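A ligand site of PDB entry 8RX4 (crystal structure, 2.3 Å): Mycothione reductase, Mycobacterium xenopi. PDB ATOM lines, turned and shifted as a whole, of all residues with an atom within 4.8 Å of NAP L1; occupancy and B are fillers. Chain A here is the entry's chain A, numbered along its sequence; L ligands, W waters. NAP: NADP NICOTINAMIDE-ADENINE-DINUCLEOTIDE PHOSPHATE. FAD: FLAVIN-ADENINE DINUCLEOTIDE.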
ATOM      1  N   LYS A  48     -21.234  29.066 -16.638  1.00  0.00           N
ATOM      2  CA  LYS A  48     -20.736  30.016 -17.626  1.00  0.00           C
ATOM      3  C   LYS A  48     -21.169  31.432 -17.292  1.00  0.00           C
ATOM      4  O   LYS A  48     -20.403  32.375 -17.520  1.00  0.00           O
ATOM      5  CB  LYS A  48     -21.217  29.617 -19.022  1.00  0.00           C
ATOM      6  CG  LYS A  48     -20.168  28.884 -19.837  1.00  0.00           C
ATOM      7  CD  LYS A  48     -19.370  27.890 -18.977  1.00  0.00           C
ATOM      8  CE  LYS A  48     -20.123  26.592 -18.745  1.00  0.00           C
ATOM      9  NZ  LYS A  48     -19.246  25.494 -18.216  1.00  0.00           N
ATOM     10  N   PRO A 149     -13.240  10.864  -3.703  1.00  0.00           N
ATOM     11  CA  PRO A 149     -12.259   9.875  -3.294  1.00  0.00           C
ATOM     12  C   PRO A 149     -12.578   9.353  -1.914  1.00  0.00           C
ATOM     13  O   PRO A 149     -13.110  10.080  -1.054  1.00  0.00           O
ATOM     14  CB  PRO A 149     -10.939  10.651  -3.317  1.00  0.00           C
ATOM     15  CG  PRO A 149     -11.329  12.082  -3.191  1.00  0.00           C
ATOM     16  CD  PRO A 149     -12.642  12.201  -3.896  1.00  0.00           C
ATOM     17  N   VAL A 178      -9.544  19.641  -5.197  1.00  0.00           N
ATOM     18  CA  VAL A 178      -8.919  18.340  -5.418  1.00  0.00           C
ATOM     19  C   VAL A 178      -9.328  17.867  -6.798  1.00  0.00           C
ATOM     20  O   VAL A 178     -10.517  17.832  -7.121  1.00  0.00           O
ATOM     21  CB  VAL A 178      -9.333  17.320  -4.337  1.00  0.00           C
ATOM     22  CG1 VAL A 178      -8.564  16.038  -4.526  1.00  0.00           C
ATOM     23  CG2 VAL A 178      -9.084  17.895  -2.962  1.00  0.00           C
ATOM     24  N   GLY A 179      -8.340  17.507  -7.610  1.00  0.00           N
ATOM     25  CA  GLY A 179      -8.569  17.124  -8.992  1.00  0.00           C
ATOM     26  C   GLY A 179      -8.132  18.226  -9.954  1.00  0.00           C
ATOM     27  O   GLY A 179      -7.991  19.395  -9.593  1.00  0.00           O
ATOM     28  N   GLY A 180      -7.902  17.819 -11.200  1.00  0.00           N
ATOM     29  CA  GLY A 180      -7.493  18.776 -12.215  1.00  0.00           C
ATOM     30  C   GLY A 180      -8.128  18.527 -13.570  1.00  0.00           C
ATOM     31  O   GLY A 180      -7.423  18.430 -14.583  1.00  0.00           O
ATOM     32  N   GLY A 181      -9.449  18.417 -13.602  1.00  0.00           N
ATOM     33  CA  GLY A 181     -10.167  18.209 -14.853  1.00  0.00           C
ATOM     34  C   GLY A 181     -10.921  19.435 -15.318  1.00  0.00           C
ATOM     35  O   GLY A 181     -10.579  20.570 -14.943  1.00  0.00           O
ATOM     36  N   PHE A 182     -11.990  19.224 -16.109  1.00  0.00           N
ATOM     37  CA  PHE A 182     -12.760  20.341 -16.647  1.00  0.00           C
ATOM     38  C   PHE A 182     -13.371  21.185 -15.541  1.00  0.00           C
ATOM     39  O   PHE A 182     -13.331  22.417 -15.593  1.00  0.00           O
ATOM     40  CB  PHE A 182     -13.875  19.825 -17.568  1.00  0.00           C
ATOM     41  CG  PHE A 182     -13.406  19.446 -18.955  1.00  0.00           C
ATOM     42  CD1 PHE A 182     -12.259  18.685 -19.154  1.00  0.00           C
ATOM     43  CD2 PHE A 182     -14.152  19.827 -20.080  1.00  0.00           C
ATOM     44  CE1 PHE A 182     -11.837  18.330 -20.435  1.00  0.00           C
ATOM     45  CE2 PHE A 182     -13.739  19.466 -21.361  1.00  0.00           C
ATOM     46  CZ  PHE A 182     -12.577  18.720 -21.538  1.00  0.00           C
ATOM     47  N   VAL A 183     -13.930  20.536 -14.514  1.00  0.00           N
ATOM     48  CA  VAL A 183     -14.577  21.268 -13.436  1.00  0.00           C
ATOM     49  C   VAL A 183     -13.544  22.054 -12.641  1.00  0.00           C
ATOM     50  O   VAL A 183     -13.787  23.212 -12.261  1.00  0.00           O
ATOM     51  CB  VAL A 183     -15.369  20.310 -12.522  1.00  0.00           C
ATOM     52  CG1 VAL A 183     -15.989  21.061 -11.345  1.00  0.00           C
ATOM     53  CG2 VAL A 183     -16.442  19.588 -13.301  1.00  0.00           C
ATOM     54  N   ALA A 184     -12.376  21.469 -12.392  1.00  0.00           N
ATOM     55  CA  ALA A 184     -11.361  22.152 -11.597  1.00  0.00           C
ATOM     56  C   ALA A 184     -10.855  23.402 -12.288  1.00  0.00           C
ATOM     57  O   ALA A 184     -10.755  24.465 -11.669  1.00  0.00           O
ATOM     58  CB  ALA A 184     -10.192  21.198 -11.302  1.00  0.00           C
ATOM     59  N   GLU A 186     -12.300  25.328 -14.604  1.00  0.00           N
ATOM     60  CA  GLU A 186     -13.306  26.372 -14.692  1.00  0.00           C
ATOM     61  C   GLU A 186     -13.523  27.042 -13.338  1.00  0.00           C
ATOM     62  O   GLU A 186     -13.506  28.280 -13.238  1.00  0.00           O
ATOM     63  CB  GLU A 186     -14.617  25.793 -15.230  1.00  0.00           C
ATOM     64  CG  GLU A 186     -14.484  25.105 -16.593  1.00  0.00           C
ATOM     65  CD  GLU A 186     -15.795  24.904 -17.347  1.00  0.00           C
ATOM     66  OE1 GLU A 186     -16.860  24.726 -16.724  1.00  0.00           O
ATOM     67  OE2 GLU A 186     -15.756  24.925 -18.603  1.00  0.00           O
ATOM     68  N   ARG A 203      -3.478  14.240  -8.402  1.00  0.00           N
ATOM     69  CA  ARG A 203      -2.686  13.030  -8.287  1.00  0.00           C
ATOM     70  C   ARG A 203      -1.700  12.878  -9.431  1.00  0.00           C
ATOM     71  O   ARG A 203      -0.777  12.057  -9.323  1.00  0.00           O
ATOM     72  CB  ARG A 203      -3.613  11.812  -8.204  1.00  0.00           C
ATOM     73  CG  ARG A 203      -4.023  11.248  -9.549  1.00  0.00           C
ATOM     74  CD  ARG A 203      -5.476  10.808  -9.577  1.00  0.00           C
ATOM     75  NE  ARG A 203      -5.705   9.615  -8.763  1.00  0.00           N
ATOM     76  CZ  ARG A 203      -6.700   8.765  -8.955  1.00  0.00           C
ATOM     77  NH1 ARG A 203      -7.577   8.932  -9.937  1.00  0.00           N
ATOM     78  NH2 ARG A 203      -6.829   7.712  -8.145  1.00  0.00           N
ATOM     79  N   GLY A 204      -1.851  13.648 -10.504  1.00  0.00           N
ATOM     80  CA  GLY A 204      -0.935  13.625 -11.622  1.00  0.00           C
ATOM     81  C   GLY A 204      -0.008  14.830 -11.607  1.00  0.00           C
ATOM     82  O   GLY A 204       0.100  15.585 -10.638  1.00  0.00           O
ATOM     83  N   ARG A 209      -5.577  16.623 -18.522  1.00  0.00           N
ATOM     84  CA  ARG A 209      -4.621  15.592 -18.920  1.00  0.00           C
ATOM     85  C   ARG A 209      -4.874  15.097 -20.338  1.00  0.00           C
ATOM     86  O   ARG A 209      -3.930  14.809 -21.075  1.00  0.00           O
ATOM     87  CB  ARG A 209      -4.696  14.428 -17.925  1.00  0.00           C
ATOM     88  CG  ARG A 209      -3.629  13.386 -18.106  1.00  0.00           C
ATOM     89  CD  ARG A 209      -3.434  12.556 -16.835  1.00  0.00           C
ATOM     90  NE  ARG A 209      -4.667  11.908 -16.382  1.00  0.00           N
ATOM     91  CZ  ARG A 209      -5.193  10.827 -16.942  1.00  0.00           C
ATOM     92  NH1 ARG A 209      -4.627  10.260 -17.998  1.00  0.00           N
ATOM     93  NH2 ARG A 209      -6.299  10.300 -16.418  1.00  0.00           N
ATOM     94  N   ASN A 234      -2.155  12.666  -3.400  1.00  0.00           N
ATOM     95  CA  ASN A 234      -3.494  12.234  -3.046  1.00  0.00           C
ATOM     96  C   ASN A 234      -3.813  12.695  -1.629  1.00  0.00           C
ATOM     97  O   ASN A 234      -2.922  12.942  -0.819  1.00  0.00           O
ATOM     98  CB  ASN A 234      -3.638  10.712  -3.131  1.00  0.00           C
ATOM     99  CG  ASN A 234      -3.372  10.187  -4.513  1.00  0.00           C
ATOM    100  OD1 ASN A 234      -2.226  10.155  -4.975  1.00  0.00           O
ATOM    101  ND2 ASN A 234      -4.436   9.753  -5.203  1.00  0.00           N
ATOM    102  N   ALA A 263     -13.395  18.087  -7.244  1.00  0.00           N
ATOM    103  CA  ALA A 263     -13.688  18.006  -8.665  1.00  0.00           C
ATOM    104  C   ALA A 263     -12.971  16.801  -9.256  1.00  0.00           C
ATOM    105  O   ALA A 263     -12.124  16.953 -10.139  1.00  0.00           O
ATOM    106  CB  ALA A 263     -13.260  19.301  -9.367  1.00  0.00           C
ATOM    107  N   THR A 264     -13.292  15.605  -8.769  1.00  0.00           N
ATOM    108  CA  THR A 264     -12.575  14.392  -9.140  1.00  0.00           C
ATOM    109  C   THR A 264     -13.416  13.489 -10.034  1.00  0.00           C
ATOM    110  O   THR A 264     -13.413  12.270  -9.885  1.00  0.00           O
ATOM    111  CB  THR A 264     -12.117  13.634  -7.901  1.00  0.00           C
ATOM    112  OG1 THR A 264     -13.228  13.431  -7.013  1.00  0.00           O
ATOM    113  CG2 THR A 264     -11.031  14.424  -7.189  1.00  0.00           C
ATOM    114  N   GLY A 265     -14.171  14.097 -10.960  1.00  0.00           N
ATOM    115  CA  GLY A 265     -14.943  13.341 -11.926  1.00  0.00           C
ATOM    116  C   GLY A 265     -16.359  13.072 -11.458  1.00  0.00           C
ATOM    117  O   GLY A 265     -16.760  13.423 -10.343  1.00  0.00           O
ATOM    118  N   ARG A 266     -17.135  12.455 -12.354  1.00  0.00           N
ATOM    119  CA  ARG A 266     -18.505  12.067 -12.079  1.00  0.00           C
ATOM    120  C   ARG A 266     -18.700  10.592 -12.434  1.00  0.00           C
ATOM    121  O   ARG A 266     -17.894   9.984 -13.137  1.00  0.00           O
ATOM    122  CB  ARG A 266     -19.528  12.916 -12.867  1.00  0.00           C
ATOM    123  CG  ARG A 266     -19.100  14.327 -13.152  1.00  0.00           C
ATOM    124  CD  ARG A 266     -20.019  15.366 -12.529  1.00  0.00           C
ATOM    125  NE  ARG A 266     -21.425  15.099 -12.782  1.00  0.00           N
ATOM    126  CZ  ARG A 266     -22.415  15.749 -12.179  1.00  0.00           C
ATOM    127  NH1 ARG A 266     -22.191  16.689 -11.275  1.00  0.00           N
ATOM    128  NH2 ARG A 266     -23.676  15.419 -12.471  1.00  0.00           N
ATOM    129  N   GLU A 311     -19.570  13.235 -21.694  1.00  0.00           N
ATOM    130  CA  GLU A 311     -20.357  13.994 -20.715  1.00  0.00           C
ATOM    131  C   GLU A 311     -20.489  15.434 -21.204  1.00  0.00           C
ATOM    132  O   GLU A 311     -19.912  16.380 -20.660  1.00  0.00           O
ATOM    133  CB  GLU A 311     -19.705  13.922 -19.341  1.00  0.00           C
ATOM    134  CG  GLU A 311     -19.421  12.507 -18.821  1.00  0.00           C
ATOM    135  CD  GLU A 311     -19.500  12.378 -17.293  1.00  0.00           C
ATOM    136  OE1 GLU A 311     -20.000  13.304 -16.618  1.00  0.00           O
ATOM    137  OE2 GLU A 311     -19.052  11.337 -16.769  1.00  0.00           O
ATOM    138  N   LEU A 312     -21.272  15.598 -22.273  1.00  0.00           N
ATOM    139  CA  LEU A 312     -21.438  16.878 -22.923  1.00  0.00           C
ATOM    140  C   LEU A 312     -22.903  17.087 -23.278  1.00  0.00           C
ATOM    141  O   LEU A 312     -23.568  16.170 -23.776  1.00  0.00           O
ATOM    142  CB  LEU A 312     -20.556  16.973 -24.184  1.00  0.00           C
ATOM    143  CG  LEU A 312     -19.058  16.783 -23.930  1.00  0.00           C
ATOM    144  CD1 LEU A 312     -18.369  16.110 -25.107  1.00  0.00           C
ATOM    145  CD2 LEU A 312     -18.385  18.106 -23.576  1.00  0.00           C
ATOM    146  N   ALA A 348     -15.047  22.187 -24.944  1.00  0.00           N
ATOM    147  CA  ALA A 348     -14.410  23.438 -24.543  1.00  0.00           C
ATOM    148  C   ALA A 348     -14.317  23.485 -23.015  1.00  0.00           C
ATOM    149  O   ALA A 348     -15.157  22.924 -22.311  1.00  0.00           O
ATOM    150  CB  ALA A 348     -15.207  24.652 -25.055  1.00  0.00           C
ATOM    151  N   VAL A 349     -13.278  24.152 -22.530  1.00  0.00           N
ATOM    152  CA  VAL A 349     -13.097  24.371 -21.094  1.00  0.00           C
ATOM    153  C   VAL A 349     -13.088  25.871 -20.857  1.00  0.00           C
ATOM    154  O   VAL A 349     -12.205  26.581 -21.352  1.00  0.00           O
ATOM    155  CB  VAL A 349     -11.815  23.717 -20.562  1.00  0.00           C
ATOM    156  CG1 VAL A 349     -11.780  23.798 -19.055  1.00  0.00           C
ATOM    157  CG2 VAL A 349     -11.743  22.266 -21.017  1.00  0.00           C
ATOM    158  N   PHE A 350     -14.080  26.364 -20.111  1.00  0.00           N
ATOM    159  CA  PHE A 350     -14.220  27.798 -19.900  1.00  0.00           C
ATOM    160  C   PHE A 350     -13.367  28.217 -18.701  1.00  0.00           C
ATOM    161  O   PHE A 350     -13.848  28.707 -17.673  1.00  0.00           O
ATOM    162  CB  PHE A 350     -15.692  28.173 -19.749  1.00  0.00           C
ATOM    163  CG  PHE A 350     -16.472  28.042 -21.037  1.00  0.00           C
ATOM    164  CD1 PHE A 350     -16.942  26.807 -21.459  1.00  0.00           C
ATOM    165  CD2 PHE A 350     -16.686  29.148 -21.854  1.00  0.00           C
ATOM    166  CE1 PHE A 350     -17.634  26.675 -22.648  1.00  0.00           C
ATOM    167  CE2 PHE A 350     -17.386  29.027 -23.041  1.00  0.00           C
ATOM    168  CZ  PHE A 350     -17.851  27.784 -23.443  1.00  0.00           C
HETATM  169  PA  NAP L   1     -12.719  15.006 -15.438  1.00  0.00           P
HETATM  170  O1A NAP L   1     -12.898  13.594 -15.866  1.00  0.00           O
HETATM  171  O2A NAP L   1     -12.755  16.081 -16.480  1.00  0.00           O
HETATM  172  O5B NAP L   1     -11.368  15.150 -14.578  1.00  0.00           O
HETATM  173  C5B NAP L   1     -11.316  14.433 -13.313  1.00  0.00           C
HETATM  174  C4B NAP L   1     -10.100  14.838 -12.518  1.00  0.00           C
HETATM  175  O4B NAP L   1     -10.230  14.241 -11.190  1.00  0.00           O
HETATM  176  C3B NAP L   1      -8.741  14.360 -13.039  1.00  0.00           C
HETATM  177  O3B NAP L   1      -7.750  15.350 -12.778  1.00  0.00           O
HETATM  178  C2B NAP L   1      -8.509  13.097 -12.223  1.00  0.00           C
HETATM  179  O2B NAP L   1      -7.141  12.714 -12.081  1.00  0.00           O
HETATM  180  C1B NAP L   1      -9.052  13.552 -10.880  1.00  0.00           C
HETATM  181  N9A NAP L   1      -9.402  12.440  -9.991  1.00  0.00           N
HETATM  182  C8A NAP L   1     -10.311  11.453 -10.259  1.00  0.00           C
HETATM  183  N7A NAP L   1     -10.430  10.578  -9.299  1.00  0.00           N
HETATM  184  C5A NAP L   1      -9.524  11.014  -8.331  1.00  0.00           C
HETATM  185  C6A NAP L   1      -9.173  10.497  -7.068  1.00  0.00           C
HETATM  186  N6A NAP L   1      -9.716   9.407  -6.537  1.00  0.00           N
HETATM  187  N1A NAP L   1      -8.236  11.168  -6.360  1.00  0.00           N
HETATM  188  C2A NAP L   1      -7.702  12.271  -6.903  1.00  0.00           C
HETATM  189  N3A NAP L   1      -7.940  12.839  -8.078  1.00  0.00           N
HETATM  190  C4A NAP L   1      -8.883  12.160  -8.758  1.00  0.00           C
HETATM  191  O3  NAP L   1     -13.808  15.337 -14.291  1.00  0.00           O
HETATM  192  PN  NAP L   1     -14.503  16.703 -13.837  1.00  0.00           P
HETATM  193  O1N NAP L   1     -15.144  16.532 -12.504  1.00  0.00           O
HETATM  194  O2N NAP L   1     -13.519  17.808 -14.050  1.00  0.00           O
HETATM  195  O5D NAP L   1     -15.662  16.803 -14.949  1.00  0.00           O
HETATM  196  C5D NAP L   1     -16.674  15.768 -14.934  1.00  0.00           C
HETATM  197  C4D NAP L   1     -17.278  15.600 -16.306  1.00  0.00           C
HETATM  198  O4D NAP L   1     -18.000  16.798 -16.677  1.00  0.00           O
HETATM  199  C3D NAP L   1     -16.299  15.310 -17.460  1.00  0.00           C
HETATM  200  O3D NAP L   1     -16.807  14.330 -18.349  1.00  0.00           O
HETATM  201  C2D NAP L   1     -16.141  16.675 -18.139  1.00  0.00           C
HETATM  202  O2D NAP L   1     -15.873  16.591 -19.524  1.00  0.00           O
HETATM  203  C1D NAP L   1     -17.532  17.279 -17.931  1.00  0.00           C
HETATM  204  N1N NAP L   1     -17.479  18.757 -17.877  1.00  0.00           N
HETATM  205  C2N NAP L   1     -17.481  19.475 -19.047  1.00  0.00           C
HETATM  206  C3N NAP L   1     -17.384  20.865 -19.005  1.00  0.00           C
HETATM  207  C7N NAP L   1     -17.409  21.613 -20.305  1.00  0.00           C
HETATM  208  O7N NAP L   1     -17.545  20.971 -21.361  1.00  0.00           O
HETATM  209  N7N NAP L   1     -17.269  22.933 -20.287  1.00  0.00           N
HETATM  210  C4N NAP L   1     -17.286  21.518 -17.780  1.00  0.00           C
HETATM  211  C5N NAP L   1     -17.282  20.777 -16.620  1.00  0.00           C
HETATM  212  C6N NAP L   1     -17.366  19.405 -16.669  1.00  0.00           C
HETATM  213  P2B NAP L   1      -6.668  11.676 -13.213  1.00  0.00           P
HETATM  214  O1X NAP L   1      -5.229  11.342 -12.860  1.00  0.00           O
HETATM  215  O2X NAP L   1      -6.786  12.380 -14.559  1.00  0.00           O
HETATM  216  O3X NAP L   1      -7.586  10.462 -13.116  1.00  0.00           O
HETATM  217  PA  FAD L   2     -28.866  15.278 -16.041  1.00  0.00           P
HETATM  218  O1A FAD L   2     -29.087  16.653 -16.534  1.00  0.00           O
HETATM  219  O2A FAD L   2     -28.034  15.199 -14.755  1.00  0.00           O
HETATM  220  O5B FAD L   2     -30.256  14.528 -15.860  1.00  0.00           O
HETATM  221  C5B FAD L   2     -30.449  13.551 -14.809  1.00  0.00           C
HETATM  222  C4B FAD L   2     -31.600  13.983 -13.933  1.00  0.00           C
HETATM  223  O4B FAD L   2     -32.359  12.837 -13.502  1.00  0.00           O
HETATM  224  C3B FAD L   2     -31.182  14.714 -12.659  1.00  0.00           C
HETATM  225  O3B FAD L   2     -32.099  15.770 -12.377  1.00  0.00           O
HETATM  226  C2B FAD L   2     -31.224  13.613 -11.605  1.00  0.00           C
HETATM  227  O2B FAD L   2     -31.465  14.133 -10.312  1.00  0.00           O
HETATM  228  C1B FAD L   2     -32.409  12.786 -12.091  1.00  0.00           C
HETATM  229  N9A FAD L   2     -32.402  11.388 -11.680  1.00  0.00           N
HETATM  230  C8A FAD L   2     -31.315  10.548 -11.659  1.00  0.00           C
HETATM  231  N7A FAD L   2     -31.581   9.334 -11.265  1.00  0.00           N
HETATM  232  C5A FAD L   2     -32.942   9.357 -10.997  1.00  0.00           C
HETATM  233  C6A FAD L   2     -33.847   8.385 -10.537  1.00  0.00           C
HETATM  234  N6A FAD L   2     -33.492   7.124 -10.245  1.00  0.00           N
HETATM  235  N1A FAD L   2     -35.143   8.745 -10.381  1.00  0.00           N
HETATM  236  C2A FAD L   2     -35.493   9.999 -10.667  1.00  0.00           C
HETATM  237  N3A FAD L   2     -34.728  11.006 -11.104  1.00  0.00           N
HETATM  238  C4A FAD L   2     -33.462  10.617 -11.252  1.00  0.00           C
HETATM  239  N1  FAD L   2     -21.517  20.136 -20.755  1.00  0.00           N
HETATM  240  C2  FAD L   2     -21.315  20.968 -21.819  1.00  0.00           C
HETATM  241  O2  FAD L   2     -21.570  20.620 -22.981  1.00  0.00           O
HETATM  242  N3  FAD L   2     -20.818  22.243 -21.616  1.00  0.00           N
HETATM  243  C4  FAD L   2     -20.491  22.798 -20.400  1.00  0.00           C
HETATM  244  O4  FAD L   2     -20.050  23.948 -20.339  1.00  0.00           O
HETATM  245  C4X FAD L   2     -20.705  21.914 -19.268  1.00  0.00           C
HETATM  246  N5  FAD L   2     -20.417  22.363 -18.071  1.00  0.00           N
HETATM  247  C5X FAD L   2     -20.615  21.505 -16.989  1.00  0.00           C
HETATM  248  C6  FAD L   2     -20.314  21.957 -15.700  1.00  0.00           C
HETATM  249  C7  FAD L   2     -20.503  21.143 -14.593  1.00  0.00           C
HETATM  250  C7M FAD L   2     -20.158  21.661 -13.217  1.00  0.00           C
HETATM  251  C8  FAD L   2     -21.002  19.837 -14.762  1.00  0.00           C
HETATM  252  C8M FAD L   2     -21.222  18.927 -13.590  1.00  0.00           C
HETATM  253  C9  FAD L   2     -21.303  19.385 -16.051  1.00  0.00           C
HETATM  254  C9A FAD L   2     -21.117  20.204 -17.150  1.00  0.00           C
HETATM  255  N10 FAD L   2     -21.403  19.766 -18.467  1.00  0.00           N
HETATM  256  C10 FAD L   2     -21.218  20.606 -19.543  1.00  0.00           C
HETATM  257  C1' FAD L   2     -21.946  18.432 -18.699  1.00  0.00           C
HETATM  258  C2' FAD L   2     -23.465  18.439 -18.839  1.00  0.00           C
HETATM  259  O2' FAD L   2     -24.057  19.194 -17.792  1.00  0.00           O
HETATM  260  C3' FAD L   2     -23.992  17.001 -18.804  1.00  0.00           C
HETATM  261  O3' FAD L   2     -23.415  16.286 -19.895  1.00  0.00           O
HETATM  262  C4' FAD L   2     -25.507  16.931 -18.915  1.00  0.00           C
HETATM  263  O4' FAD L   2     -26.113  17.600 -17.804  1.00  0.00           O
HETATM  264  C5' FAD L   2     -26.034  15.523 -19.027  1.00  0.00           C
HETATM  265  O5' FAD L   2     -27.457  15.581 -19.214  1.00  0.00           O
HETATM  266  P   FAD L   2     -28.387  14.427 -18.718  1.00  0.00           P
HETATM  267  O1P FAD L   2     -29.852  14.771 -18.961  1.00  0.00           O
HETATM  268  O2P FAD L   2     -27.813  13.203 -19.340  1.00  0.00           O
HETATM  269  O3P FAD L   2     -28.133  14.411 -17.146  1.00  0.00           O
HETATM  270  O   HOH W   1      -6.234  14.707  -9.330  1.00  0.00           O
HETATM  271  O   HOH W   2     -11.926  18.744 -12.473  1.00  0.00           O
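NZ of Lys 48 lies within hydrogen-bond range of O4 of FAD L2 (2.7 Å). The backbone NH of Leu 312 sits at hydrogen-bond distance from an oxygen (O3') of FAD L2, at 3.3 Å. NH1 of Arg 203 is in salt-bridge range of O3X of NAP L1 (3.5 Å). O3B of NAP L1 sits at hydrogen-bond distance from N of Gly 180 (2.9 Å). OE2 of Glu 186 lies within hydrogen-bond range of N7N of NAP L1, at 3.0 Å. NH2 of Arg 209 is in salt-bridge range of O2X of NAP L1, 2.8 Å away. An oxygen (O2N) of NAP L1 is in hydrogen-bond range of the backbone NH of Phe 182. O of Ala 348 lies within hydrogen-bond range of N7N of NAP L1 (2.9 Å). The backbone NH of Val 183 lies within hydrogen-bond range of an oxygen (O2N) of NAP L1 (2.8 Å). The backbone NH (N) of Gly 265 is in hydrogen-bond range of an oxygen (O1N) of NAP L1, at 3.0 Å.
A nitrogen (N7N) of NAP L1 sits at hydrogen-bond distance from an oxygen (O4) of FAD L2, at 3.0 Å.
The backbone NH (N) of Phe 350 lies within hydrogen-bond range of the side-chain carboxylate (OE2) of Glu 186, 2.7 Å away. The side-chain carboxylate (OE1) of Glu 186 lies within salt-bridge range of the side-chain amino group (NZ) of Lys 48 (2.9 Å). O of Val 178 sits at hydrogen-bond distance from N of Ala 263 (2.9 Å).
Water W1 lies within hydrogen-bond range of N3A of NAP L1 (2.8 Å) and N of Arg 203 (2.9 Å).
An oxygen (O4B) of NAP L1 lies close to the backbone carbonyl oxygen (O) of Ala 263 (3.5 Å). O of Thr 264 lies close to N7A of NAP L1, at 3.5 Å. Residues that only touch NAP L1: Glu 311, Gly 181, Arg 266, Pro 149, Leu 312, Lys 48 and Gly 179. Hydrophobic or aromatic side chains within 4 Å of NAP L1: Pro 149, Phe 182, Val 183 and Leu 312.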
